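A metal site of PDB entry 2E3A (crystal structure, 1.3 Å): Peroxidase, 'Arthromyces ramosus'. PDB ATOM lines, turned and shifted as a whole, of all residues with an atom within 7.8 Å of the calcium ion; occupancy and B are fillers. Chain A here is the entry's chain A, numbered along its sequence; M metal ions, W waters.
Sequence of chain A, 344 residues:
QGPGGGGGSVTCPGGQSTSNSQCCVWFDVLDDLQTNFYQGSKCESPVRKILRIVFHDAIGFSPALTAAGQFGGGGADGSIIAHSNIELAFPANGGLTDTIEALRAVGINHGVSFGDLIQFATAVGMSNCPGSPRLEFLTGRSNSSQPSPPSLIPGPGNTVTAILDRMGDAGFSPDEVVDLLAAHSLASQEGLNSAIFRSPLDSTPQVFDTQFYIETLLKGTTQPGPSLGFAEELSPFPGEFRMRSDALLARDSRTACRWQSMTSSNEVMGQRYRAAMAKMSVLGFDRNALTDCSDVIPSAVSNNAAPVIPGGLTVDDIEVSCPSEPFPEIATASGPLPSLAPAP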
ATOM      1  N   ILE A  53     -14.087  -4.219  15.075  1.00  0.00           N
ATOM      2  CA  ILE A  53     -14.877  -4.879  16.112  1.00  0.00           C
ATOM      3  C   ILE A  53     -15.210  -3.967  17.274  1.00  0.00           C
ATOM      4  O   ILE A  53     -16.336  -4.004  17.766  1.00  0.00           O
ATOM      5  CB  ILE A  53     -14.190  -6.182  16.570  1.00  0.00           C
ATOM      6  CG1 ILE A  53     -14.198  -7.212  15.428  1.00  0.00           C
ATOM      7  CG2 ILE A  53     -14.770  -6.683  17.878  1.00  0.00           C
ATOM      8  CD1 ILE A  53     -13.239  -8.361  15.588  1.00  0.00           C
ATOM      9  N   VAL A  54     -14.299  -3.093  17.688  1.00  0.00           N
ATOM     10  CA  VAL A  54     -14.578  -2.233  18.836  1.00  0.00           C
ATOM     11  C   VAL A  54     -15.674  -1.242  18.483  1.00  0.00           C
ATOM     12  O   VAL A  54     -16.582  -0.976  19.256  1.00  0.00           O
ATOM     13  CB  VAL A  54     -13.305  -1.571  19.386  1.00  0.00           C
ATOM     14  CG1 VAL A  54     -12.757  -0.490  18.458  1.00  0.00           C
ATOM     15  CG2 VAL A  54     -13.518  -1.014  20.786  1.00  0.00           C
ATOM     16  N   PHE A  55     -15.614  -0.693  17.299  1.00  0.00           N
ATOM     17  CA  PHE A  55     -16.626   0.211  16.808  1.00  0.00           C
ATOM     18  C   PHE A  55     -17.951  -0.524  16.668  1.00  0.00           C
ATOM     19  O   PHE A  55     -19.008  -0.053  17.129  1.00  0.00           O
ATOM     20  CB  PHE A  55     -16.179   0.827  15.500  1.00  0.00           C
ATOM     21  CG  PHE A  55     -17.176   1.755  14.818  1.00  0.00           C
ATOM     22  CD1 PHE A  55     -17.989   2.632  15.524  1.00  0.00           C
ATOM     23  CD2 PHE A  55     -17.302   1.721  13.444  1.00  0.00           C
ATOM     24  CE1 PHE A  55     -18.885   3.465  14.893  1.00  0.00           C
ATOM     25  CE2 PHE A  55     -18.201   2.562  12.791  1.00  0.00           C
ATOM     26  CZ  PHE A  55     -19.008   3.435  13.511  1.00  0.00           C
ATOM     27  N   HIS A  56     -17.959  -1.686  16.041  1.00  0.00           N
ATOM     28  CA  HIS A  56     -19.231  -2.358  15.798  1.00  0.00           C
ATOM     29  C   HIS A  56     -19.812  -3.017  17.028  1.00  0.00           C
ATOM     30  O   HIS A  56     -21.020  -3.275  17.105  1.00  0.00           O
ATOM     31  CB  HIS A  56     -19.087  -3.366  14.665  1.00  0.00           C
ATOM     32  CG  HIS A  56     -18.697  -2.767  13.362  1.00  0.00           C
ATOM     33  ND1 HIS A  56     -18.612  -3.481  12.186  1.00  0.00           N
ATOM     34  CD2 HIS A  56     -18.363  -1.468  13.060  1.00  0.00           C
ATOM     35  CE1 HIS A  56     -18.241  -2.653  11.226  1.00  0.00           C
ATOM     36  NE2 HIS A  56     -18.079  -1.465  11.728  1.00  0.00           N
ATOM     37  N   ASP A  57     -19.000  -3.264  18.049  1.00  0.00           N
ATOM     38  CA  ASP A  57     -19.562  -3.632  19.351  1.00  0.00           C
ATOM     39  C   ASP A  57     -20.210  -2.423  20.012  1.00  0.00           C
ATOM     40  O   ASP A  57     -21.378  -2.531  20.379  1.00  0.00           O
ATOM     41  CB  ASP A  57     -18.486  -4.259  20.248  1.00  0.00           C
ATOM     42  CG  ASP A  57     -19.113  -4.781  21.525  1.00  0.00           C
ATOM     43  OD1 ASP A  57     -20.242  -5.284  21.434  1.00  0.00           O
ATOM     44  OD2 ASP A  57     -18.477  -4.752  22.598  1.00  0.00           O
ATOM     45  N   ALA A  58     -19.505  -1.312  20.141  1.00  0.00           N
ATOM     46  CA  ALA A  58     -19.962  -0.167  20.907  1.00  0.00           C
ATOM     47  C   ALA A  58     -21.148   0.556  20.282  1.00  0.00           C
ATOM     48  O   ALA A  58     -22.011   1.039  21.001  1.00  0.00           O
ATOM     49  CB  ALA A  58     -18.813   0.816  21.132  1.00  0.00           C
ATOM     50  N   ILE A  59     -21.180   0.622  18.947  1.00  0.00           N
ATOM     51  CA  ILE A  59     -22.149   1.460  18.254  1.00  0.00           C
ATOM     52  C   ILE A  59     -23.516   0.805  18.287  1.00  0.00           C
ATOM     53  O   ILE A  59     -24.467   1.490  17.889  1.00  0.00           O
ATOM     54  CB  ILE A  59     -21.668   1.794  16.836  1.00  0.00           C
ATOM     55  CG1 ILE A  59     -22.178   3.162  16.324  1.00  0.00           C
ATOM     56  CG2 ILE A  59     -21.990   0.714  15.806  1.00  0.00           C
ATOM     57  CD1 ILE A  59     -21.854   4.315  17.252  1.00  0.00           C
ATOM     58  N   GLY A  60     -23.626  -0.453  18.738  1.00  0.00           N
ATOM     59  CA  GLY A  60     -24.967  -1.022  18.900  1.00  0.00           C
ATOM     60  C   GLY A  60     -25.572  -0.536  20.219  1.00  0.00           C
ATOM     61  O   GLY A  60     -25.654  -1.217  21.221  1.00  0.00           O
ATOM     62  N   PHE A  61     -25.964   0.735  20.114  1.00  0.00           N
ATOM     63  CA  PHE A  61     -26.440   1.498  21.262  1.00  0.00           C
ATOM     64  C   PHE A  61     -27.289   2.609  20.655  1.00  0.00           C
ATOM     65  O   PHE A  61     -26.817   3.389  19.852  1.00  0.00           O
ATOM     66  CB  PHE A  61     -25.278   2.012  22.087  1.00  0.00           C
ATOM     67  CG  PHE A  61     -25.692   2.813  23.296  1.00  0.00           C
ATOM     68  CD1 PHE A  61     -26.153   2.178  24.423  1.00  0.00           C
ATOM     69  CD2 PHE A  61     -25.628   4.194  23.310  1.00  0.00           C
ATOM     70  CE1 PHE A  61     -26.584   2.836  25.557  1.00  0.00           C
ATOM     71  CE2 PHE A  61     -26.076   4.881  24.418  1.00  0.00           C
ATOM     72  CZ  PHE A  61     -26.528   4.215  25.542  1.00  0.00           C
ATOM     73  N   GLY A  73     -29.870  -1.759  22.449  1.00  0.00           N
ATOM     74  CA  GLY A  73     -28.501  -2.243  22.497  1.00  0.00           C
ATOM     75  C   GLY A  73     -27.752  -1.845  23.754  1.00  0.00           C
ATOM     76  O   GLY A  73     -27.986  -0.828  24.358  1.00  0.00           O
ATOM     77  N   GLY A  74     -26.786  -2.678  24.149  1.00  0.00           N
ATOM     78  CA  GLY A  74     -26.027  -2.462  25.341  1.00  0.00           C
ATOM     79  C   GLY A  74     -24.668  -1.843  25.144  1.00  0.00           C
ATOM     80  O   GLY A  74     -23.894  -1.787  26.099  1.00  0.00           O
ATOM     81  N   GLY A  75     -24.369  -1.357  23.932  1.00  0.00           N
ATOM     82  CA  GLY A  75     -23.094  -0.633  23.759  1.00  0.00           C
ATOM     83  C   GLY A  75     -21.895  -1.585  23.750  1.00  0.00           C
ATOM     84  O   GLY A  75     -21.904  -2.651  23.123  1.00  0.00           O
ATOM     85  N   ALA A  76     -20.884  -1.213  24.487  1.00  0.00           N
ATOM     86  CA  ALA A  76     -19.586  -1.888  24.559  1.00  0.00           C
ATOM     87  C   ALA A  76     -19.642  -3.165  25.393  1.00  0.00           C
ATOM     88  O   ALA A  76     -18.830  -3.358  26.325  1.00  0.00           O
ATOM     89  CB  ALA A  76     -18.564  -0.918  25.091  1.00  0.00           C
ATOM     90  N   ASP A  77     -20.603  -4.013  25.103  1.00  0.00           N
ATOM     91  CA  ASP A  77     -21.008  -5.116  25.969  1.00  0.00           C
ATOM     92  C   ASP A  77     -20.508  -6.459  25.516  1.00  0.00           C
ATOM     93  O   ASP A  77     -20.864  -7.498  26.067  1.00  0.00           O
ATOM     94  CB  ASP A  77     -22.524  -5.149  26.041  1.00  0.00           C
ATOM     95  CG  ASP A  77     -23.263  -5.255  24.740  1.00  0.00           C
ATOM     96  OD1 ASP A  77     -22.625  -5.367  23.666  1.00  0.00           O
ATOM     97  OD2 ASP A  77     -24.533  -5.258  24.774  1.00  0.00           O
ATOM     98  N   GLY A  78     -19.691  -6.492  24.461  1.00  0.00           N
ATOM     99  CA  GLY A  78     -19.210  -7.812  23.990  1.00  0.00           C
ATOM    100  C   GLY A  78     -20.247  -8.568  23.192  1.00  0.00           C
ATOM    101  O   GLY A  78     -20.011  -9.710  22.858  1.00  0.00           O
ATOM    102  N   SER A  79     -21.380  -7.958  22.864  1.00  0.00           N
ATOM    103  CA  SER A  79     -22.449  -8.656  22.167  1.00  0.00           C
ATOM    104  C   SER A  79     -22.067  -9.186  20.785  1.00  0.00           C
ATOM    105  O   SER A  79     -22.572 -10.211  20.374  1.00  0.00           O
ATOM    106  CB  SER A  79     -23.685  -7.765  22.034  1.00  0.00           C
ATOM    107  OG  SER A  79     -23.450  -6.656  21.157  1.00  0.00           O
ATOM    108  N   ILE A  80     -21.122  -8.499  20.162  1.00  0.00           N
ATOM    109  CA  ILE A  80     -20.674  -8.903  18.838  1.00  0.00           C
ATOM    110  C   ILE A  80     -19.993 -10.275  18.947  1.00  0.00           C
ATOM    111  O   ILE A  80     -19.950 -11.039  17.936  1.00  0.00           O
ATOM    112  CB  ILE A  80     -19.801  -7.815  18.187  1.00  0.00           C
ATOM    113  CG1 ILE A  80     -19.607  -8.083  16.693  1.00  0.00           C
ATOM    114  CG2 ILE A  80     -18.484  -7.669  18.954  1.00  0.00           C
ATOM    115  CD1 ILE A  80     -18.937  -6.939  15.940  1.00  0.00           C
ATOM    116  N   ILE A  81     -19.416 -10.618  20.105  1.00  0.00           N
ATOM    117  CA  ILE A  81     -18.889 -11.966  20.361  1.00  0.00           C
ATOM    118  C   ILE A  81     -19.945 -12.873  20.923  1.00  0.00           C
ATOM    119  O   ILE A  81     -20.195 -13.972  20.372  1.00  0.00           O
ATOM    120  CB  ILE A  81     -17.651 -11.934  21.262  1.00  0.00           C
ATOM    121  CG1 ILE A  81     -16.527 -11.029  20.724  1.00  0.00           C
ATOM    122  CG2 ILE A  81     -17.131 -13.324  21.550  1.00  0.00           C
ATOM    123  CD1 ILE A  81     -15.311 -10.864  21.629  1.00  0.00           C
ATOM    124  N   GLU A  87     -25.064 -11.046  15.140  1.00  0.00           N
ATOM    125  CA  GLU A  87     -24.490  -9.806  14.677  1.00  0.00           C
ATOM    126  C   GLU A  87     -23.597  -9.979  13.458  1.00  0.00           C
ATOM    127  O   GLU A  87     -23.504  -9.005  12.691  1.00  0.00           O
ATOM    128  CB  GLU A  87     -23.707  -9.139  15.835  1.00  0.00           C
ATOM    129  CG  GLU A  87     -24.612  -8.805  17.005  1.00  0.00           C
ATOM    130  CD  GLU A  87     -24.056  -7.798  17.999  1.00  0.00           C
ATOM    131  OE1 GLU A  87     -23.154  -7.022  17.632  1.00  0.00           O
ATOM    132  OE2 GLU A  87     -24.562  -7.796  19.138  1.00  0.00           O
ATOM    133  N   GLY A 115     -16.810  -7.757  26.610  1.00  0.00           N
ATOM    134  CA  GLY A 115     -16.799  -6.318  26.391  1.00  0.00           C
ATOM    135  C   GLY A 115     -15.480  -5.720  26.841  1.00  0.00           C
ATOM    136  O   GLY A 115     -14.900  -4.868  26.152  1.00  0.00           O
ATOM    137  N   ILE A 118     -12.608  -6.742  24.283  1.00  0.00           N
ATOM    138  CA  ILE A 118     -12.555  -6.007  23.029  1.00  0.00           C
ATOM    139  C   ILE A 118     -11.863  -4.668  23.252  1.00  0.00           C
ATOM    140  O   ILE A 118     -11.000  -4.232  22.484  1.00  0.00           O
ATOM    141  CB  ILE A 118     -13.918  -5.827  22.395  1.00  0.00           C
ATOM    142  CG1 ILE A 118     -14.446  -7.199  21.925  1.00  0.00           C
ATOM    143  CG2 ILE A 118     -13.968  -4.816  21.272  1.00  0.00           C
ATOM    144  CD1 ILE A 118     -15.910  -7.196  21.537  1.00  0.00           C
ATOM    145  N   SER A 145     -24.811  -9.865  27.880  1.00  0.00           N
ATOM    146  CA  SER A 145     -25.337  -9.017  26.809  1.00  0.00           C
ATOM    147  C   SER A 145     -26.545  -9.629  26.116  1.00  0.00           C
ATOM    148  O   SER A 145     -26.707 -10.835  26.142  1.00  0.00           O
ATOM    149  CB  SER A 145     -24.244  -8.773  25.763  1.00  0.00           C
ATOM    150  OG  SER A 145     -23.854  -9.961  25.120  1.00  0.00           O
ATOM    151  N   GLN A 146     -27.323  -8.777  25.491  1.00  0.00           N
ATOM    152  CA  GLN A 146     -28.360  -9.161  24.547  1.00  0.00           C
ATOM    153  C   GLN A 146     -27.847  -8.843  23.144  1.00  0.00           C
ATOM    154  O   GLN A 146     -26.954  -7.988  23.038  1.00  0.00           O
ATOM    155  CB  GLN A 146     -29.672  -8.432  24.782  1.00  0.00           C
ATOM    156  CG  GLN A 146     -30.429  -8.768  26.044  1.00  0.00           C
ATOM    157  CD  GLN A 146     -31.265  -7.556  26.448  1.00  0.00           C
ATOM    158  OE1 GLN A 146     -30.860  -6.866  27.391  1.00  0.00           O
ATOM    159  NE2 GLN A 146     -32.373  -7.261  25.760  1.00  0.00           N
ATOM    160  N   PRO A 147     -28.378  -9.430  22.083  1.00  0.00           N
ATOM    161  CA  PRO A 147     -27.889  -9.089  20.736  1.00  0.00           C
ATOM    162  C   PRO A 147     -28.152  -7.624  20.431  1.00  0.00           C
ATOM    163  O   PRO A 147     -29.220  -7.120  20.810  1.00  0.00           O
ATOM    164  CB  PRO A 147     -28.733  -9.952  19.802  1.00  0.00           C
ATOM    165  CG  PRO A 147     -29.233 -11.087  20.663  1.00  0.00           C
ATOM    166  CD  PRO A 147     -29.446 -10.457  22.010  1.00  0.00           C
ATOM    167  N   SER A 148     -27.206  -6.974  19.759  1.00  0.00           N
ATOM    168  CA  SER A 148     -27.501  -5.652  19.211  1.00  0.00           C
ATOM    169  C   SER A 148     -28.720  -5.662  18.307  1.00  0.00           C
ATOM    170  O   SER A 148     -28.830  -6.588  17.482  1.00  0.00           O
ATOM    171  CB  SER A 148     -26.311  -5.167  18.372  1.00  0.00           C
ATOM    172  OG  SER A 148     -26.584  -3.868  17.817  1.00  0.00           O
ATOM    173  N   PRO A 149     -29.566  -4.644  18.341  1.00  0.00           N
ATOM    174  CA  PRO A 149     -30.545  -4.456  17.268  1.00  0.00           C
ATOM    175  C   PRO A 149     -29.784  -4.344  15.949  1.00  0.00           C
ATOM    176  O   PRO A 149     -28.608  -3.955  15.895  1.00  0.00           O
ATOM    177  CB  PRO A 149     -31.221  -3.146  17.634  1.00  0.00           C
ATOM    178  CG  PRO A 149     -31.045  -3.075  19.113  1.00  0.00           C
ATOM    179  CD  PRO A 149     -29.687  -3.665  19.401  1.00  0.00           C
ATOM    180  N   LEU A 283     -20.078   3.335  26.117  1.00  0.00           N
ATOM    181  CA  LEU A 283     -21.486   3.341  25.753  1.00  0.00           C
ATOM    182  C   LEU A 283     -22.103   2.117  26.398  1.00  0.00           C
ATOM    183  O   LEU A 283     -21.612   1.000  26.227  1.00  0.00           O
ATOM    184  CB  LEU A 283     -21.650   3.356  24.234  1.00  0.00           C
ATOM    185  CG  LEU A 283     -21.136   4.601  23.489  1.00  0.00           C
ATOM    186  CD1 LEU A 283     -21.429   4.369  21.998  1.00  0.00           C
ATOM    187  CD2 LEU A 283     -21.816   5.878  23.919  1.00  0.00           C
ATOM    188  N   PHE A 285     -22.476   1.865  29.741  1.00  0.00           N
ATOM    189  CA  PHE A 285     -21.854   1.746  31.038  1.00  0.00           C
ATOM    190  C   PHE A 285     -21.599   3.069  31.737  1.00  0.00           C
ATOM    191  O   PHE A 285     -21.500   4.120  31.097  1.00  0.00           O
ATOM    192  CB  PHE A 285     -20.487   1.031  30.933  1.00  0.00           C
ATOM    193  CG  PHE A 285     -20.696  -0.349  30.326  1.00  0.00           C
ATOM    194  CD1 PHE A 285     -20.657  -0.529  28.970  1.00  0.00           C
ATOM    195  CD2 PHE A 285     -21.002  -1.434  31.130  1.00  0.00           C
ATOM    196  CE1 PHE A 285     -20.936  -1.768  28.429  1.00  0.00           C
ATOM    197  CE2 PHE A 285     -21.210  -2.670  30.605  1.00  0.00           C
ATOM    198  CZ  PHE A 285     -21.200  -2.847  29.239  1.00  0.00           C
HETATM  199 CA    CA M   1     -22.449  -4.438  21.509  1.00  0.00          CA
HETATM  200  O   HOH W   1     -24.675  -3.732  21.295  1.00  0.00           O
HETATM  201  O   HOH W   2     -22.636  -4.811  19.062  1.00  0.00           O
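The side-chain carboxylate (OD2) of Asp 77 lies close to the backbone NH (N) of Gly 74 (3.5 Å). OD2 of Asp 57 is in hydrogen-bond range of N of Gly 78 (2.8 Å). The side-chain carboxylate (OE2) of Glu 87 lies close to the side-chain hydroxyl (OG) of Ser 79 (2.6 Å). The backbone NH (N) of Gly 75 sits at hydrogen-bond distance from the backbone carbonyl oxygen (O) of Gly 60 (3.0 Å).
Within 4 Å of the calcium ion: Asp 57, Gly 75, Asp 77 and Ser 79. Along chain A the residues within 4 Å of the calcium ion span positions 57 to 79.
The calcium ion is bound by water W1 (2.3 Å), OD1 of Asp 77 (2.4 Å), OD1 of Asp 57 (2.4 Å), OG of Ser 79 (2.5 Å), O of Asp 57 (2.5 Å), O of Gly 75 (2.5 Å) and water W2 (2.5 Å).
Water W2 lies within hydrogen-bond range of OE1 of Glu 87 and O of His 56.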
